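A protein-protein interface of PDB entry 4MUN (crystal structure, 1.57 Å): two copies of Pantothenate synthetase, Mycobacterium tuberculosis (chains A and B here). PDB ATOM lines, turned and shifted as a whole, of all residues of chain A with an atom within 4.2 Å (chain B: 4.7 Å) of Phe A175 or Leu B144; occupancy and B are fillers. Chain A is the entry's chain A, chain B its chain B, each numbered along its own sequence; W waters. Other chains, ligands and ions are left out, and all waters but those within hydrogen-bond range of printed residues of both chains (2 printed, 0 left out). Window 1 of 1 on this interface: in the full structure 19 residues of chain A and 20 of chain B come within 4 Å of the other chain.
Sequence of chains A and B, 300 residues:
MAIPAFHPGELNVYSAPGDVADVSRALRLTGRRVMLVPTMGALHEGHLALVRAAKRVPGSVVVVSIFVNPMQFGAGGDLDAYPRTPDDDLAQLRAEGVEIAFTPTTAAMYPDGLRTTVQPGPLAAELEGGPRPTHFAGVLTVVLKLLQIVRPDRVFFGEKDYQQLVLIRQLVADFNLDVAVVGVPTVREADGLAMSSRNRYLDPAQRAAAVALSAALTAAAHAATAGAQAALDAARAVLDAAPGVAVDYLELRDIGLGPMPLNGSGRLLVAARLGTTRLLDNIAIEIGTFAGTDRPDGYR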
ATOM      1  N   VAL A 118     -26.249  -9.989  12.439  1.00  0.00           N
ATOM      2  CA  VAL A 118     -25.731 -11.308  12.070  1.00  0.00           C
ATOM      3  C   VAL A 118     -26.515 -12.343  12.753  1.00  0.00           C
ATOM      4  O   VAL A 118     -26.698 -12.341  13.960  1.00  0.00           O
ATOM      5  CB  VAL A 118     -24.249 -11.466  12.404  1.00  0.00           C
ATOM      6  CG1 VAL A 118     -23.799 -12.846  11.938  1.00  0.00           C
ATOM      7  CG2 VAL A 118     -23.425 -10.394  11.679  1.00  0.00           C
ATOM      8  N   LEU A 171     -18.166 -17.133  11.210  1.00  0.00           N
ATOM      9  CA  LEU A 171     -18.454 -15.841  10.615  1.00  0.00           C
ATOM     10  C   LEU A 171     -17.477 -15.517   9.488  1.00  0.00           C
ATOM     11  O   LEU A 171     -17.856 -15.106   8.378  1.00  0.00           O
ATOM     12  CB  LEU A 171     -18.341 -14.800  11.733  1.00  0.00           C
ATOM     13  CG  LEU A 171     -18.398 -13.337  11.380  1.00  0.00           C
ATOM     14  CD1 LEU A 171     -19.801 -12.862  11.045  1.00  0.00           C
ATOM     15  CD2 LEU A 171     -17.878 -12.352  12.415  1.00  0.00           C
ATOM     16  N   VAL A 172     -16.182 -15.678   9.796  1.00  0.00           N
ATOM     17  CA  VAL A 172     -15.117 -15.397   8.888  1.00  0.00           C
ATOM     18  C   VAL A 172     -15.241 -16.218   7.601  1.00  0.00           C
ATOM     19  O   VAL A 172     -15.139 -15.672   6.461  1.00  0.00           O
ATOM     20  CB  VAL A 172     -13.767 -15.412   9.595  1.00  0.00           C
ATOM     21  CG1 VAL A 172     -12.646 -15.397   8.600  1.00  0.00           C
ATOM     22  CG2 VAL A 172     -13.731 -14.239  10.562  1.00  0.00           C
ATOM     23  N   ALA A 173     -15.443 -17.516   7.776  1.00  0.00           N
ATOM     24  CA  ALA A 173     -15.615 -18.418   6.619  1.00  0.00           C
ATOM     25  C   ALA A 173     -16.864 -18.062   5.818  1.00  0.00           C
ATOM     26  O   ALA A 173     -16.826 -17.986   4.553  1.00  0.00           O
ATOM     27  CB  ALA A 173     -15.629 -19.886   7.039  1.00  0.00           C
ATOM     28  N   ASP A 174     -17.989 -17.941   6.496  1.00  0.00           N
ATOM     29  CA  ASP A 174     -19.288 -17.870   5.928  1.00  0.00           C
ATOM     30  C   ASP A 174     -19.549 -16.572   5.171  1.00  0.00           C
ATOM     31  O   ASP A 174     -20.293 -16.520   4.211  1.00  0.00           O
ATOM     32  CB  ASP A 174     -20.373 -18.108   6.967  1.00  0.00           C
ATOM     33  CG  ASP A 174     -20.380 -19.519   7.502  1.00  0.00           C
ATOM     34  OD1 ASP A 174     -19.661 -20.372   6.929  1.00  0.00           O
ATOM     35  OD2 ASP A 174     -21.060 -19.711   8.526  1.00  0.00           O
ATOM     36  N   PHE A 175     -18.894 -15.489   5.655  1.00  0.00           N
ATOM     37  CA  PHE A 175     -19.042 -14.220   4.935  1.00  0.00           C
ATOM     38  C   PHE A 175     -17.734 -13.842   4.153  1.00  0.00           C
ATOM     39  O   PHE A 175     -17.591 -12.708   3.678  1.00  0.00           O
ATOM     40  CB  PHE A 175     -19.307 -13.133   5.960  1.00  0.00           C
ATOM     41  CG  PHE A 175     -20.651 -13.187   6.604  1.00  0.00           C
ATOM     42  CD1 PHE A 175     -21.697 -14.014   6.129  1.00  0.00           C
ATOM     43  CD2 PHE A 175     -20.947 -12.402   7.677  1.00  0.00           C
ATOM     44  CE1 PHE A 175     -22.938 -13.949   6.694  1.00  0.00           C
ATOM     45  CE2 PHE A 175     -22.197 -12.355   8.270  1.00  0.00           C
ATOM     46  CZ  PHE A 175     -23.217 -13.137   7.772  1.00  0.00           C
ATOM     47  N   ASN A 176     -16.816 -14.805   3.916  1.00  0.00           N
ATOM     48  CA  ASN A 176     -15.655 -14.613   3.056  1.00  0.00           C
ATOM     49  C   ASN A 176     -14.828 -13.444   3.572  1.00  0.00           C
ATOM     50  O   ASN A 176     -14.319 -12.702   2.735  1.00  0.00           O
ATOM     51  CB  ASN A 176     -16.133 -14.358   1.633  1.00  0.00           C
ATOM     52  CG  ASN A 176     -16.959 -15.491   1.072  1.00  0.00           C
ATOM     53  OD1 ASN A 176     -18.177 -15.503   1.195  1.00  0.00           O
ATOM     54  ND2 ASN A 176     -16.288 -16.468   0.512  1.00  0.00           N
ATOM     55  N   LEU A 177     -14.716 -13.296   4.895  1.00  0.00           N
ATOM     56  CA  LEU A 177     -13.891 -12.154   5.410  1.00  0.00           C
ATOM     57  C   LEU A 177     -12.442 -12.419   5.215  1.00  0.00           C
ATOM     58  O   LEU A 177     -11.945 -13.510   5.379  1.00  0.00           O
ATOM     59  CB  LEU A 177     -14.228 -11.813   6.807  1.00  0.00           C
ATOM     60  CG  LEU A 177     -15.690 -11.664   7.219  1.00  0.00           C
ATOM     61  CD1 LEU A 177     -15.904 -11.501   8.727  1.00  0.00           C
ATOM     62  CD2 LEU A 177     -16.396 -10.602   6.480  1.00  0.00           C
ATOM     63  N   THR B 116     -23.986 -19.136   8.884  1.00  0.00           N
ATOM     64  CA  THR B 116     -24.129 -17.742   9.369  1.00  0.00           C
ATOM     65  C   THR B 116     -24.802 -16.962   8.236  1.00  0.00           C
ATOM     66  O   THR B 116     -24.414 -17.136   7.027  1.00  0.00           O
ATOM     67  CB  THR B 116     -22.764 -17.091   9.542  1.00  0.00           C
ATOM     68  OG1 THR B 116     -21.850 -17.951  10.279  1.00  0.00           O
ATOM     69  CG2 THR B 116     -22.906 -15.776  10.313  1.00  0.00           C
ATOM     70  N   THR B 117     -25.813 -16.201   8.575  1.00  0.00           N
ATOM     71  CA  THR B 117     -26.535 -15.422   7.571  1.00  0.00           C
ATOM     72  C   THR B 117     -26.752 -14.019   8.031  1.00  0.00           C
ATOM     73  O   THR B 117     -26.475 -13.660   9.182  1.00  0.00           O
ATOM     74  CB  THR B 117     -27.908 -16.111   7.252  1.00  0.00           C
ATOM     75  OG1 THR B 117     -28.761 -16.079   8.379  1.00  0.00           O
ATOM     76  CG2 THR B 117     -27.676 -17.498   6.558  1.00  0.00           C
ATOM     77  N   VAL B 118     -27.226 -13.175   7.104  1.00  0.00           N
ATOM     78  CA  VAL B 118     -27.600 -11.798   7.514  1.00  0.00           C
ATOM     79  C   VAL B 118     -29.088 -11.690   7.858  1.00  0.00           C
ATOM     80  O   VAL B 118     -29.912 -12.222   7.140  1.00  0.00           O
ATOM     81  CB  VAL B 118     -27.298 -10.785   6.410  1.00  0.00           C
ATOM     82  CG1 VAL B 118     -27.732  -9.387   6.873  1.00  0.00           C
ATOM     83  CG2 VAL B 118     -25.795 -10.788   6.000  1.00  0.00           C
ATOM     84  N   LEU B 140     -29.398 -10.124   1.113  1.00  0.00           N
ATOM     85  CA  LEU B 140     -28.350  -9.429   1.872  1.00  0.00           C
ATOM     86  C   LEU B 140     -27.188 -10.338   2.214  1.00  0.00           C
ATOM     87  O   LEU B 140     -26.043  -9.899   2.211  1.00  0.00           O
ATOM     88  CB  LEU B 140     -28.901  -8.808   3.125  1.00  0.00           C
ATOM     89  CG  LEU B 140     -29.790  -7.600   3.080  1.00  0.00           C
ATOM     90  CD1 LEU B 140     -29.892  -6.820   4.393  1.00  0.00           C
ATOM     91  CD2 LEU B 140     -29.448  -6.685   1.953  1.00  0.00           C
ATOM     92  N   THR B 141     -27.419 -11.600   2.470  1.00  0.00           N
ATOM     93  CA  THR B 141     -26.374 -12.598   2.677  1.00  0.00           C
ATOM     94  C   THR B 141     -25.453 -12.755   1.457  1.00  0.00           C
ATOM     95  O   THR B 141     -24.205 -12.648   1.522  1.00  0.00           O
ATOM     96  CB  THR B 141     -26.952 -13.958   3.161  1.00  0.00           C
ATOM     97  OG1 THR B 141     -27.738 -13.785   4.373  1.00  0.00           O
ATOM     98  CG2 THR B 141     -25.872 -14.907   3.394  1.00  0.00           C
ATOM     99  N   VAL B 142     -26.052 -12.904   0.269  1.00  0.00           N
ATOM    100  CA  VAL B 142     -25.237 -13.028  -0.912  1.00  0.00           C
ATOM    101  C   VAL B 142     -24.514 -11.754  -1.268  1.00  0.00           C
ATOM    102  O   VAL B 142     -23.313 -11.792  -1.624  1.00  0.00           O
ATOM    103  CB  VAL B 142     -26.085 -13.615  -2.092  1.00  0.00           C
ATOM    104  CG1 VAL B 142     -27.008 -12.572  -2.762  1.00  0.00           C
ATOM    105  CG2 VAL B 142     -25.138 -14.294  -3.075  1.00  0.00           C
ATOM    106  N   VAL B 143     -25.191 -10.618  -1.123  1.00  0.00           N
ATOM    107  CA  VAL B 143     -24.561  -9.308  -1.440  1.00  0.00           C
ATOM    108  C   VAL B 143     -23.371  -9.116  -0.465  1.00  0.00           C
ATOM    109  O   VAL B 143     -22.291  -8.665  -0.896  1.00  0.00           O
ATOM    110  CB  VAL B 143     -25.548  -8.175  -1.420  1.00  0.00           C
ATOM    111  CG1 VAL B 143     -24.836  -6.865  -1.405  1.00  0.00           C
ATOM    112  CG2 VAL B 143     -26.529  -8.298  -2.597  1.00  0.00           C
ATOM    113  N   LEU B 144     -23.560  -9.463   0.803  1.00  0.00           N
ATOM    114  CA  LEU B 144     -22.416  -9.295   1.716  1.00  0.00           C
ATOM    115  C   LEU B 144     -21.184 -10.111   1.311  1.00  0.00           C
ATOM    116  O   LEU B 144     -20.078  -9.639   1.277  1.00  0.00           O
ATOM    117  CB  LEU B 144     -22.831  -9.631   3.170  1.00  0.00           C
ATOM    118  CG  LEU B 144     -21.733  -9.545   4.234  1.00  0.00           C
ATOM    119  CD1 LEU B 144     -21.090  -8.166   4.287  1.00  0.00           C
ATOM    120  CD2 LEU B 144     -22.299  -9.993   5.551  1.00  0.00           C
ATOM    121  N   LYS B 145     -21.452 -11.375   0.957  1.00  0.00           N
ATOM    122  CA  LYS B 145     -20.424 -12.264   0.493  1.00  0.00           C
ATOM    123  C   LYS B 145     -19.710 -11.767  -0.748  1.00  0.00           C
ATOM    124  O   LYS B 145     -18.518 -11.748  -0.831  1.00  0.00           O
ATOM    125  CB  LYS B 145     -21.033 -13.651   0.315  1.00  0.00           C
ATOM    126  CG  LYS B 145     -21.405 -14.313   1.699  1.00  0.00           C
ATOM    127  CD  LYS B 145     -22.228 -15.615   1.487  1.00  0.00           C
ATOM    128  CE  LYS B 145     -21.464 -16.655   0.705  1.00  0.00           C
ATOM    129  NZ  LYS B 145     -20.346 -17.322   1.357  1.00  0.00           N
ATOM    130  N   LEU B 146     -20.468 -11.267  -1.720  1.00  0.00           N
ATOM    131  CA  LEU B 146     -19.874 -10.766  -2.968  1.00  0.00           C
ATOM    132  C   LEU B 146     -19.029  -9.575  -2.703  1.00  0.00           C
ATOM    133  O   LEU B 146     -17.959  -9.418  -3.250  1.00  0.00           O
ATOM    134  CB  LEU B 146     -20.985 -10.436  -3.956  1.00  0.00           C
ATOM    135  CG  LEU B 146     -21.673 -11.662  -4.562  1.00  0.00           C
ATOM    136  CD1 LEU B 146     -22.936 -11.200  -5.275  1.00  0.00           C
ATOM    137  CD2 LEU B 146     -20.797 -12.431  -5.487  1.00  0.00           C
ATOM    138  N   LEU B 147     -19.508  -8.742  -1.750  1.00  0.00           N
ATOM    139  CA  LEU B 147     -18.737  -7.566  -1.375  1.00  0.00           C
ATOM    140  C   LEU B 147     -17.415  -7.926  -0.714  1.00  0.00           C
ATOM    141  O   LEU B 147     -16.389  -7.225  -0.934  1.00  0.00           O
ATOM    142  CB  LEU B 147     -19.554  -6.604  -0.503  1.00  0.00           C
ATOM    143  CG  LEU B 147     -20.668  -5.770  -1.151  1.00  0.00           C
ATOM    144  CD1 LEU B 147     -21.541  -5.079  -0.091  1.00  0.00           C
ATOM    145  CD2 LEU B 147     -20.095  -4.840  -2.206  1.00  0.00           C
ATOM    146  N   GLN B 148     -17.407  -8.955   0.099  1.00  0.00           N
ATOM    147  CA  GLN B 148     -16.198  -9.372   0.819  1.00  0.00           C
ATOM    148  C   GLN B 148     -15.227 -10.086  -0.119  1.00  0.00           C
ATOM    149  O   GLN B 148     -14.011  -9.981  -0.009  1.00  0.00           O
ATOM    150  CB  GLN B 148     -16.597 -10.251   1.981  1.00  0.00           C
ATOM    151  CG  GLN B 148     -17.408  -9.510   3.026  1.00  0.00           C
ATOM    152  CD  GLN B 148     -16.723  -8.316   3.692  1.00  0.00           C
ATOM    153  OE1 GLN B 148     -15.566  -8.346   3.938  1.00  0.00           O
ATOM    154  NE2 GLN B 148     -17.453  -7.316   3.960  1.00  0.00           N
ATOM    155  N   LEU B 171     -27.531  -2.421   5.173  1.00  0.00           N
ATOM    156  CA  LEU B 171     -26.433  -3.395   5.364  1.00  0.00           C
ATOM    157  C   LEU B 171     -25.100  -2.670   5.434  1.00  0.00           C
ATOM    158  O   LEU B 171     -24.319  -2.947   6.375  1.00  0.00           O
ATOM    159  CB  LEU B 171     -26.418  -4.376   4.199  1.00  0.00           C
ATOM    160  CG  LEU B 171     -25.247  -5.391   4.073  1.00  0.00           C
ATOM    161  CD1 LEU B 171     -25.465  -6.512   5.035  1.00  0.00           C
ATOM    162  CD2 LEU B 171     -25.152  -5.972   2.652  1.00  0.00           C
ATOM    163  N   PHE B 175     -23.100  -2.535   9.027  1.00  0.00           N
ATOM    164  CA  PHE B 175     -21.919  -3.329   9.267  1.00  0.00           C
ATOM    165  C   PHE B 175     -20.624  -2.575   8.925  1.00  0.00           C
ATOM    166  O   PHE B 175     -19.568  -3.161   8.817  1.00  0.00           O
ATOM    167  CB  PHE B 175     -21.994  -4.609   8.400  1.00  0.00           C
ATOM    168  CG  PHE B 175     -23.040  -5.592   8.798  1.00  0.00           C
ATOM    169  CD1 PHE B 175     -23.692  -5.590  10.042  1.00  0.00           C
ATOM    170  CD2 PHE B 175     -23.351  -6.571   7.937  1.00  0.00           C
ATOM    171  CE1 PHE B 175     -24.637  -6.508  10.385  1.00  0.00           C
ATOM    172  CE2 PHE B 175     -24.278  -7.504   8.268  1.00  0.00           C
ATOM    173  CZ  PHE B 175     -24.906  -7.502   9.507  1.00  0.00           C
ATOM    174  N   LEU B 177     -19.448  -1.197   6.195  1.00  0.00           N
ATOM    175  CA  LEU B 177     -18.735  -1.569   4.996  1.00  0.00           C
ATOM    176  C   LEU B 177     -18.164  -0.373   4.266  1.00  0.00           C
ATOM    177  O   LEU B 177     -18.768   0.673   4.236  1.00  0.00           O
ATOM    178  CB  LEU B 177     -19.624  -2.391   4.072  1.00  0.00           C
ATOM    179  CG  LEU B 177     -20.407  -3.540   4.671  1.00  0.00           C
ATOM    180  CD1 LEU B 177     -21.257  -4.379   3.661  1.00  0.00           C
ATOM    181  CD2 LEU B 177     -19.627  -4.533   5.483  1.00  0.00           C
HETATM  182  O   HOH W   1     -18.233 -19.248   2.579  1.00  0.00           O
HETATM  183  O   HOH W   2     -12.392 -12.644   0.816  1.00  0.00           O
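Val A118 touches Phe B175, and with the chains exchanged Phe A175 touches Val B118. Positions printed for both chains: 118, 171, 175 and 177. Of the 14 pairs that touch across the chains among the printed residues, 2 have their exchanged pair printed and touching as well.
Of the 8 printed residues of chain A, 6 touch a printed residue of chain B. Hydrophobic or aromatic side chains of chain A within 4 Å of the printed part of chain B: Val A118, Phe A175 and Leu A177. Along chain B the printed residues that touch a printed residue of chain A span positions 116 to 175. Among the printed residues, 14 pairs touch across the chains. Among the printed residues, no Asp or Glu carboxylate lies within 4 Å of a Lys or Arg side-chain nitrogen of the other chain.
Water W2 bridges the backbone carbonyl oxygen of Asn A176 and the backbone carbonyl oxygen of Gln B148. Water W1 lies within hydrogen-bond range of O of Ala A173 (2.7 Å) and NZ of Lys B145 (3.1 Å).
The backbone NH of Leu A177 sits at hydrogen-bond distance from the backbone carbonyl oxygen of Val A172 (2.9 Å). The backbone NH (N) of Val B118 is in hydrogen-bond range of the side-chain hydroxyl (OG1) of Thr B141, at 2.8 Å.
Printed residues of chain A within 4 Å of Val B118: Phe A175 (3.9 Å). Of the printed residues of chain A, Lys B145 touches Asp A174 (3.0 Å) and Asn A176 (2.8 Å). Of the printed residues of chain A, Gln B148 touches Phe A175 (3.1 Å), Asn A176 (3.4 Å) and Leu A177 (3.5 Å). Val B143 touches none of the printed residues of chain A. Ala A173 touches none of the printed residues of chain B. The nearest printed residue of chain A that does not touch Phe B175 is Phe A175 (5.3 Å).
Thr B116 touches Val A118. Val A118 touches Thr B117. Val A118 touches Phe B175. Thr B116 touches Leu A171. Thr B116 touches Phe A175. Thr B117 touches Phe A175. Val B118 touches Phe A175 (CG2 to CZ, 3.9 Å). Gln B148 touches Phe A175 (CB to O, 3.1 Å). Asn A176 touches Gln B148 (O to CB, 3.4 Å). Leu A177 touches Gln B148 (CD2 to OE1, 3.5 Å).
The side-chain hydroxyl (OG1) of Thr B116 sits at hydrogen-bond distance from the side-chain carboxylate (OD2) of Asp A174, at 2.6 Å. The backbone carbonyl oxygen (O) of Asp A174 is in hydrogen-bond range of the side-chain amino group (NZ) of Lys B145 (3.0 Å). The side-chain amino group (NZ) of Lys B145 is in hydrogen-bond range of the side-chain amide oxygen (OD1) of Asn A176, 2.8 Å away.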
